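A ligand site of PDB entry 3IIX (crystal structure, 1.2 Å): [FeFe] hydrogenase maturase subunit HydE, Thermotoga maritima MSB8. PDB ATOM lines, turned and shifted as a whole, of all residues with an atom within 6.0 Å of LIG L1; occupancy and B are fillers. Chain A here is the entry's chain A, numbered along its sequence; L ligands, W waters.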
ATOM      1  N   TYR A  69     -24.050 -26.058 -14.846  1.00  0.00           N
ATOM      2  CA  TYR A  69     -22.941 -27.037 -14.928  1.00  0.00           C
ATOM      3  C   TYR A  69     -23.161 -28.266 -14.056  1.00  0.00           C
ATOM      4  O   TYR A  69     -22.478 -29.269 -14.249  1.00  0.00           O
ATOM      5  CB  TYR A  69     -21.624 -26.385 -14.463  1.00  0.00           C
ATOM      6  CG  TYR A  69     -21.717 -25.495 -13.251  1.00  0.00           C
ATOM      7  CD1 TYR A  69     -21.726 -26.040 -11.969  1.00  0.00           C
ATOM      8  CD2 TYR A  69     -21.825 -24.111 -13.370  1.00  0.00           C
ATOM      9  CE1 TYR A  69     -21.809 -25.236 -10.850  1.00  0.00           C
ATOM     10  CE2 TYR A  69     -21.907 -23.307 -12.250  1.00  0.00           C
ATOM     11  CZ  TYR A  69     -21.910 -23.890 -10.988  1.00  0.00           C
ATOM     12  OH  TYR A  69     -22.012 -23.043  -9.909  1.00  0.00           O
ATOM     13  N   CYS A  70     -24.117 -28.218 -13.141  1.00  0.00           N
ATOM     14  CA  CYS A  70     -24.160 -29.148 -11.991  1.00  0.00           C
ATOM     15  C   CYS A  70     -25.152 -30.279 -12.193  1.00  0.00           C
ATOM     16  O   CYS A  70     -26.325 -30.035 -12.449  1.00  0.00           O
ATOM     17  CB  CYS A  70     -24.491 -28.414 -10.682  1.00  0.00           C
ATOM     18  SG  CYS A  70     -24.449 -29.465  -9.263  1.00  0.00           S
ATOM     19  N   GLY A  71     -24.702 -31.519 -12.003  1.00  0.00           N
ATOM     20  CA  GLY A  71     -25.579 -32.643 -12.073  1.00  0.00           C
ATOM     21  C   GLY A  71     -26.678 -32.718 -11.028  1.00  0.00           C
ATOM     22  O   GLY A  71     -27.575 -33.543 -11.188  1.00  0.00           O
ATOM     23  N   GLN A 107     -21.285 -31.411   3.126  1.00  0.00           N
ATOM     24  CA  GLN A 107     -21.643 -30.764   1.870  1.00  0.00           C
ATOM     25  C   GLN A 107     -22.972 -31.310   1.371  1.00  0.00           C
ATOM     26  O   GLN A 107     -23.272 -32.480   1.536  1.00  0.00           O
ATOM     27  CB  GLN A 107     -20.578 -30.945   0.788  1.00  0.00           C
ATOM     28  CG  GLN A 107     -20.746 -30.057  -0.452  1.00  0.00           C
ATOM     29  CD  GLN A 107     -19.731 -30.331  -1.503  1.00  0.00           C
ATOM     30  OE1 GLN A 107     -19.842 -31.290  -2.272  1.00  0.00           O
ATOM     31  NE2 GLN A 107     -18.717 -29.493  -1.548  1.00  0.00           N
ATOM     32  N   SER A 136     -20.378 -26.760   3.708  1.00  0.00           N
ATOM     33  CA  SER A 136     -20.374 -26.365   2.325  1.00  0.00           C
ATOM     34  C   SER A 136     -21.801 -26.587   1.812  1.00  0.00           C
ATOM     35  O   SER A 136     -22.104 -27.579   1.153  1.00  0.00           O
ATOM     36  CB  SER A 136     -19.368 -27.201   1.538  1.00  0.00           C
ATOM     37  OG  SER A 136     -19.276 -26.857   0.176  1.00  0.00           O
ATOM     38  N   LEU A 158     -17.316 -21.978   0.014  1.00  0.00           N
ATOM     39  CA  LEU A 158     -18.292 -21.394  -0.915  1.00  0.00           C
ATOM     40  C   LEU A 158     -17.516 -20.908  -2.126  1.00  0.00           C
ATOM     41  O   LEU A 158     -17.115 -19.745  -2.179  1.00  0.00           O
ATOM     42  CB  LEU A 158     -19.049 -20.259  -0.272  1.00  0.00           C
ATOM     43  CG  LEU A 158     -20.313 -19.787  -0.980  1.00  0.00           C
ATOM     44  CD1 LEU A 158     -21.428 -20.816  -0.903  1.00  0.00           C
ATOM     45  CD2 LEU A 158     -20.789 -18.420  -0.376  1.00  0.00           C
ATOM     46  N   ARG A 159     -17.226 -21.792  -3.068  1.00  0.00           N
ATOM     47  CA  ARG A 159     -16.433 -21.397  -4.226  1.00  0.00           C
ATOM     48  C   ARG A 159     -17.113 -20.228  -4.907  1.00  0.00           C
ATOM     49  O   ARG A 159     -18.313 -20.216  -5.062  1.00  0.00           O
ATOM     50  CB  ARG A 159     -16.305 -22.539  -5.203  1.00  0.00           C
ATOM     51  CG  ARG A 159     -15.438 -23.655  -4.716  1.00  0.00           C
ATOM     52  CD  ARG A 159     -15.158 -24.539  -5.857  1.00  0.00           C
ATOM     53  NE  ARG A 159     -14.493 -25.748  -5.454  1.00  0.00           N
ATOM     54  CZ  ARG A 159     -14.153 -26.688  -6.320  1.00  0.00           C
ATOM     55  NH1 ARG A 159     -14.437 -26.540  -7.608  1.00  0.00           N
ATOM     56  NH2 ARG A 159     -13.561 -27.783  -5.896  1.00  0.00           N
ATOM     57  N   GLU A 161     -16.770 -19.583  -7.991  1.00  0.00           N
ATOM     58  CA  GLU A 161     -17.143 -20.225  -9.272  1.00  0.00           C
ATOM     59  C   GLU A 161     -16.538 -19.533 -10.488  1.00  0.00           C
ATOM     60  O   GLU A 161     -15.806 -20.139 -11.255  1.00  0.00           O
ATOM     61  CB  GLU A 161     -18.655 -20.390  -9.426  1.00  0.00           C
ATOM     62  CG  GLU A 161     -19.364 -21.065  -8.249  1.00  0.00           C
ATOM     63  CD  GLU A 161     -18.897 -22.452  -7.903  1.00  0.00           C
ATOM     64  OE1 GLU A 161     -17.922 -22.974  -8.484  1.00  0.00           O
ATOM     65  OE2 GLU A 161     -19.518 -23.032  -6.974  1.00  0.00           O
ATOM     66  N   ARG A 180     -22.895 -13.947  -4.245  1.00  0.00           N
ATOM     67  CA  ARG A 180     -21.870 -14.898  -3.839  1.00  0.00           C
ATOM     68  C   ARG A 180     -20.775 -14.209  -3.043  1.00  0.00           C
ATOM     69  O   ARG A 180     -20.351 -14.699  -2.005  1.00  0.00           O
ATOM     70  CB  ARG A 180     -21.278 -15.549  -5.086  1.00  0.00           C
ATOM     71  CG  ARG A 180     -20.533 -16.850  -4.859  1.00  0.00           C
ATOM     72  CD  ARG A 180     -21.509 -17.984  -4.554  1.00  0.00           C
ATOM     73  NE  ARG A 180     -20.882 -19.291  -4.615  1.00  0.00           N
ATOM     74  CZ  ARG A 180     -21.494 -20.440  -4.362  1.00  0.00           C
ATOM     75  NH1 ARG A 180     -22.788 -20.458  -4.061  1.00  0.00           N
ATOM     76  NH2 ARG A 180     -20.817 -21.576  -4.432  1.00  0.00           N
ATOM     77  N   SER A 198     -12.750 -21.619  -7.871  1.00  0.00           N
ATOM     78  CA  SER A 198     -13.393 -21.488  -9.152  1.00  0.00           C
ATOM     79  C   SER A 198     -13.182 -22.680 -10.023  1.00  0.00           C
ATOM     80  O   SER A 198     -12.312 -23.525  -9.763  1.00  0.00           O
ATOM     81  CB  SER A 198     -12.899 -20.234  -9.865  1.00  0.00           C
ATOM     82  OG  SER A 198     -11.484 -20.152  -9.894  1.00  0.00           O
ATOM     83  N   MET A 199     -14.001 -22.779 -11.068  1.00  0.00           N
ATOM     84  CA  MET A 199     -13.823 -23.787 -12.077  1.00  0.00           C
ATOM     85  C   MET A 199     -13.015 -23.195 -13.231  1.00  0.00           C
ATOM     86  O   MET A 199     -13.055 -21.986 -13.486  1.00  0.00           O
ATOM     87  CB  MET A 199     -15.143 -24.333 -12.573  1.00  0.00           C
ATOM     88  CG  MET A 199     -15.812 -25.282 -11.567  1.00  0.00           C
ATOM     89  SD  MET A 199     -17.461 -25.773 -12.088  1.00  0.00           S
ATOM     90  CE  MET A 199     -18.331 -24.251 -11.776  1.00  0.00           C
ATOM     91  N   GLY A 228     -10.861 -26.578  -9.620  1.00  0.00           N
ATOM     92  CA  GLY A 228     -10.881 -27.759 -10.460  1.00  0.00           C
ATOM     93  C   GLY A 228     -11.331 -27.424 -11.866  1.00  0.00           C
ATOM     94  O   GLY A 228     -11.824 -26.319 -12.108  1.00  0.00           O
ATOM     95  N   PRO A 229     -11.168 -28.373 -12.766  1.00  0.00           N
ATOM     96  CA  PRO A 229     -11.627 -28.183 -14.134  1.00  0.00           C
ATOM     97  C   PRO A 229     -13.121 -28.371 -14.210  1.00  0.00           C
ATOM     98  O   PRO A 229     -13.672 -29.194 -13.484  1.00  0.00           O
ATOM     99  CB  PRO A 229     -10.941 -29.331 -14.884  1.00  0.00           C
ATOM    100  CG  PRO A 229     -10.888 -30.403 -13.858  1.00  0.00           C
ATOM    101  CD  PRO A 229     -10.569 -29.706 -12.578  1.00  0.00           C
ATOM    102  N   PHE A 230     -13.744 -27.663 -15.135  1.00  0.00           N
ATOM    103  CA  PHE A 230     -15.125 -27.951 -15.494  1.00  0.00           C
ATOM    104  C   PHE A 230     -15.209 -29.315 -16.217  1.00  0.00           C
ATOM    105  O   PHE A 230     -14.419 -29.589 -17.123  1.00  0.00           O
ATOM    106  CB  PHE A 230     -15.678 -26.839 -16.400  1.00  0.00           C
ATOM    107  CG  PHE A 230     -16.941 -27.218 -17.120  1.00  0.00           C
ATOM    108  CD1 PHE A 230     -18.106 -27.421 -16.420  1.00  0.00           C
ATOM    109  CD2 PHE A 230     -16.941 -27.388 -18.487  1.00  0.00           C
ATOM    110  CE1 PHE A 230     -19.259 -27.814 -17.089  1.00  0.00           C
ATOM    111  CE2 PHE A 230     -18.098 -27.748 -19.146  1.00  0.00           C
ATOM    112  CZ  PHE A 230     -19.254 -27.959 -18.440  1.00  0.00           C
ATOM    113  N   ILE A 231     -16.147 -30.150 -15.788  1.00  0.00           N
ATOM    114  CA  ILE A 231     -16.354 -31.454 -16.394  1.00  0.00           C
ATOM    115  C   ILE A 231     -17.846 -31.545 -16.812  1.00  0.00           C
ATOM    116  O   ILE A 231     -18.718 -31.510 -15.931  1.00  0.00           O
ATOM    117  CB  ILE A 231     -15.977 -32.602 -15.426  1.00  0.00           C
ATOM    118  CG1 ILE A 231     -14.493 -32.532 -15.048  1.00  0.00           C
ATOM    119  CG2 ILE A 231     -16.265 -33.974 -16.072  1.00  0.00           C
ATOM    120  CD1 ILE A 231     -14.081 -33.480 -13.940  1.00  0.00           C
ATOM    121  N   PRO A 232     -18.148 -31.589 -18.129  1.00  0.00           N
ATOM    122  CA  PRO A 232     -19.558 -31.581 -18.548  1.00  0.00           C
ATOM    123  C   PRO A 232     -20.333 -32.801 -18.045  1.00  0.00           C
ATOM    124  O   PRO A 232     -19.841 -33.931 -18.058  1.00  0.00           O
ATOM    125  CB  PRO A 232     -19.468 -31.581 -20.075  1.00  0.00           C
ATOM    126  CG  PRO A 232     -18.152 -32.234 -20.366  1.00  0.00           C
ATOM    127  CD  PRO A 232     -17.248 -31.709 -19.292  1.00  0.00           C
ATOM    128  N   HIS A 233     -21.556 -32.563 -17.619  1.00  0.00           N
ATOM    129  CA  HIS A 233     -22.440 -33.601 -17.083  1.00  0.00           C
ATOM    130  C   HIS A 233     -23.563 -33.815 -18.086  1.00  0.00           C
ATOM    131  O   HIS A 233     -24.187 -32.878 -18.531  1.00  0.00           O
ATOM    132  CB  HIS A 233     -23.013 -33.157 -15.750  1.00  0.00           C
ATOM    133  CG  HIS A 233     -23.750 -34.226 -15.016  1.00  0.00           C
ATOM    134  ND1 HIS A 233     -24.922 -34.783 -15.483  1.00  0.00           N
ATOM    135  CD2 HIS A 233     -23.482 -34.847 -13.840  1.00  0.00           C
ATOM    136  CE1 HIS A 233     -25.335 -35.702 -14.619  1.00  0.00           C
ATOM    137  NE2 HIS A 233     -24.482 -35.750 -13.609  1.00  0.00           N
ATOM    138  N   ALA A 270     -12.000 -33.480  -8.764  1.00  0.00           N
ATOM    139  CA  ALA A 270     -12.149 -33.249 -10.217  1.00  0.00           C
ATOM    140  C   ALA A 270     -10.804 -33.362 -10.932  1.00  0.00           C
ATOM    141  O   ALA A 270     -10.756 -33.847 -12.066  1.00  0.00           O
ATOM    142  CB  ALA A 270     -12.832 -31.927 -10.506  1.00  0.00           C
ATOM    143  N   LEU A 305     -21.791 -34.428  -9.214  1.00  0.00           N
ATOM    144  CA  LEU A 305     -21.861 -33.082  -9.745  1.00  0.00           C
ATOM    145  C   LEU A 305     -21.407 -33.094 -11.194  1.00  0.00           C
ATOM    146  O   LEU A 305     -21.924 -32.357 -12.026  1.00  0.00           O
ATOM    147  CB  LEU A 305     -20.970 -32.145  -8.922  1.00  0.00           C
ATOM    148  CG  LEU A 305     -21.078 -32.229  -7.398  1.00  0.00           C
ATOM    149  CD1 LEU A 305     -20.282 -31.103  -6.746  1.00  0.00           C
ATOM    150  CD2 LEU A 305     -22.508 -32.205  -6.968  1.00  0.00           C
ATOM    151  N   TYR A 306     -20.414 -33.945 -11.447  1.00  0.00           N
ATOM    152  CA  TYR A 306     -19.881 -34.258 -12.764  1.00  0.00           C
ATOM    153  C   TYR A 306     -19.705 -35.783 -12.813  1.00  0.00           C
ATOM    154  O   TYR A 306     -19.608 -36.436 -11.759  1.00  0.00           O
ATOM    155  CB  TYR A 306     -18.536 -33.567 -12.976  1.00  0.00           C
ATOM    156  CG  TYR A 306     -17.573 -33.744 -11.839  1.00  0.00           C
ATOM    157  CD1 TYR A 306     -16.768 -34.877 -11.748  1.00  0.00           C
ATOM    158  CD2 TYR A 306     -17.463 -32.787 -10.841  1.00  0.00           C
ATOM    159  CE1 TYR A 306     -15.903 -35.050 -10.698  1.00  0.00           C
ATOM    160  CE2 TYR A 306     -16.588 -32.960  -9.788  1.00  0.00           C
ATOM    161  CZ  TYR A 306     -15.805 -34.089  -9.727  1.00  0.00           C
ATOM    162  OH  TYR A 306     -14.938 -34.274  -8.685  1.00  0.00           O
ATOM    163  N   PRO A 307     -19.701 -36.371 -13.996  1.00  0.00           N
ATOM    164  CA  PRO A 307     -19.527 -37.807 -14.146  1.00  0.00           C
ATOM    165  C   PRO A 307     -18.085 -38.281 -13.957  1.00  0.00           C
ATOM    166  O   PRO A 307     -17.140 -37.490 -14.077  1.00  0.00           O
ATOM    167  CB  PRO A 307     -19.953 -38.063 -15.585  1.00  0.00           C
ATOM    168  CG  PRO A 307     -19.614 -36.821 -16.302  1.00  0.00           C
ATOM    169  CD  PRO A 307     -19.865 -35.707 -15.303  1.00  0.00           C
HETATM  170  N1  LIG L   1     -17.500 -29.889 -13.157  1.00  0.00           N
HETATM  171  C1  LIG L   1     -16.503 -29.561 -12.259  1.00  0.00           C
HETATM  172  N2  LIG L   1     -16.789 -29.040 -11.040  1.00  0.00           N
HETATM  173  C2  LIG L   1     -18.087 -28.873 -10.705  1.00  0.00           C
HETATM  174  N3  LIG L   1     -18.638 -28.360  -9.580  1.00  0.00           N
HETATM  175  C3  LIG L   1     -20.000 -28.416  -9.716  1.00  0.00           C
HETATM  176  N4  LIG L   1     -20.307 -28.948 -10.919  1.00  0.00           N
HETATM  177  C4  LIG L   1     -19.133 -29.223 -11.580  1.00  0.00           C
HETATM  178  C5  LIG L   1     -18.813 -29.759 -12.806  1.00  0.00           C
HETATM  179  N5  LIG L   1     -19.745 -30.113 -13.707  1.00  0.00           N
HETATM  180  C6  LIG L   1     -17.859 -27.769  -8.479  1.00  0.00           C
HETATM  181  C7  LIG L   1     -18.302 -26.328  -8.179  1.00  0.00           C
HETATM  182  C8  LIG L   1     -18.790 -26.412  -6.747  1.00  0.00           C
HETATM  183  C9  LIG L   1     -17.922 -27.552  -6.231  1.00  0.00           C
HETATM  184  C10 LIG L   1     -18.428 -28.276  -4.996  1.00  0.00           C
HETATM  185  O1  LIG L   1     -17.959 -28.500  -7.295  1.00  0.00           O
HETATM  186  O2  LIG L   1     -17.171 -25.494  -8.326  1.00  0.00           O
HETATM  187  O3  LIG L   1     -18.591 -25.240  -5.976  1.00  0.00           O
HETATM  188  N1  LG2 L   2     -24.443 -26.374  -3.236  1.00  0.00           N
HETATM  189  C1  LG2 L   2     -23.230 -25.839  -2.566  1.00  0.00           C
HETATM  190  C2  LG2 L   2     -22.586 -24.827  -3.499  1.00  0.00           C
HETATM  191  O1  LG2 L   2     -21.708 -24.040  -3.052  1.00  0.00           O
HETATM  192  C3  LG2 L   2     -22.238 -26.970  -2.306  1.00  0.00           C
HETATM  193  C4  LG2 L   2     -21.343 -27.328  -3.470  1.00  0.00           C
HETATM  194  S1  LG2 L   2     -22.214 -27.917  -4.939  1.00  0.00           S
HETATM  195  C5  LG2 L   2     -22.797 -29.483  -4.255  1.00  0.00           C
HETATM  196  O2  LG2 L   2     -22.926 -24.769  -4.705  1.00  0.00           O
HETATM  197 FE1  LG3 L   3     -25.606 -25.166  -7.853  1.00  0.00          FE
HETATM  198 FE2  LG3 L   3     -24.325 -26.374  -5.473  1.00  0.00          FE
HETATM  199 FE3  LG3 L   3     -27.134 -26.804  -6.314  1.00  0.00          FE
HETATM  200 FE4  LG3 L   3     -25.163 -27.851  -7.804  1.00  0.00          FE
HETATM  201  S1  LG3 L   3     -25.617 -28.383  -5.659  1.00  0.00           S
HETATM  202  S2  LG3 L   3     -27.080 -26.808  -8.581  1.00  0.00           S
HETATM  203  S3  LG3 L   3     -23.547 -26.200  -7.685  1.00  0.00           S
HETATM  204  S4  LG3 L   3     -26.186 -24.801  -5.673  1.00  0.00           S
HETATM  205  O   HOH W   1     -16.580 -30.877  -6.679  1.00  0.00           O
HETATM  206  O   HOH W   2     -18.865 -24.338  -3.412  1.00  0.00           O
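Water W2 lies within hydrogen-bond range of an oxygen (O3) of LIG L1 (2.7 Å), an oxygen (O1) of LG2 L2 (2.9 Å) and the backbone NH (N) of Arg 159 (3.0 Å).
The backbone carbonyl oxygen of Ile 231 sits at hydrogen-bond distance from a nitrogen (N5) of LIG L1 (2.8 Å).
A nitrogen (N1) of LIG L1 sits at hydrogen-bond distance from the backbone NH of Ile 231 (3.0 Å).
The guanidinium group of Arg 159 lies within hydrogen-bond range of an oxygen (O2) of LIG L1, at 3.0 Å.
SD of Met 199 sits close to O2 of LIG L1, at 3.8 Å.
The guanidinium group (NH2) of Arg 180 lies within salt-bridge range of an oxygen (O1) of LG2 L2 (3.0 Å).
FE4 of LG3 L3 is bound by SG of Cys 70, at 2.3 Å.
The backbone carbonyl oxygen (O) of Tyr 69 lies within hydrogen-bond range of a nitrogen (N5) of LIG L1, 2.9 Å away.
The side-chain carboxylate (OE2) of Glu 161 is in hydrogen-bond range of an oxygen (O3) of LIG L1 (2.6 Å).
Residues that only touch LIG L1: Gln 107 (3.7 Å), Pro 229 (3.1 Å), Phe 230 (3.9 Å), Leu 305 (3.5 Å) and Tyr 306 (3.7 Å).
Hydrophobic or aromatic side chains that line LIG L1: Tyr 69, Met 199, Ile 231, Leu 305 and Tyr 306.
Of the 21 residues printed, 10 come within 4 Å of LIG L1.
FE2 of LG3 L3 is bound by N1 of LG2 L2, 2.2 Å away.
The backbone carbonyl oxygen (O) of Leu 305 lies within hydrogen-bond range of the backbone NH (N) of Gly 71.
O of Glu 161 lies within hydrogen-bond range of N of Met 199 (3.2 Å).
The guanidinium group (NH2) of Arg 180 is in salt-bridge range of the side-chain carboxylate (OE2) of Glu 161 (3.2 Å).
The side-chain hydroxyl of Tyr 306 is in hydrogen-bond range of the backbone NH of Ala 270 (3.0 Å).
The side-chain hydroxyl (OG) of Ser 136 lies within hydrogen-bond range of the side-chain amide nitrogen (NE2) of Gln 107 (3.2 Å).
O of Arg 159 is in hydrogen-bond range of NE of Arg 180 (2.8 Å).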
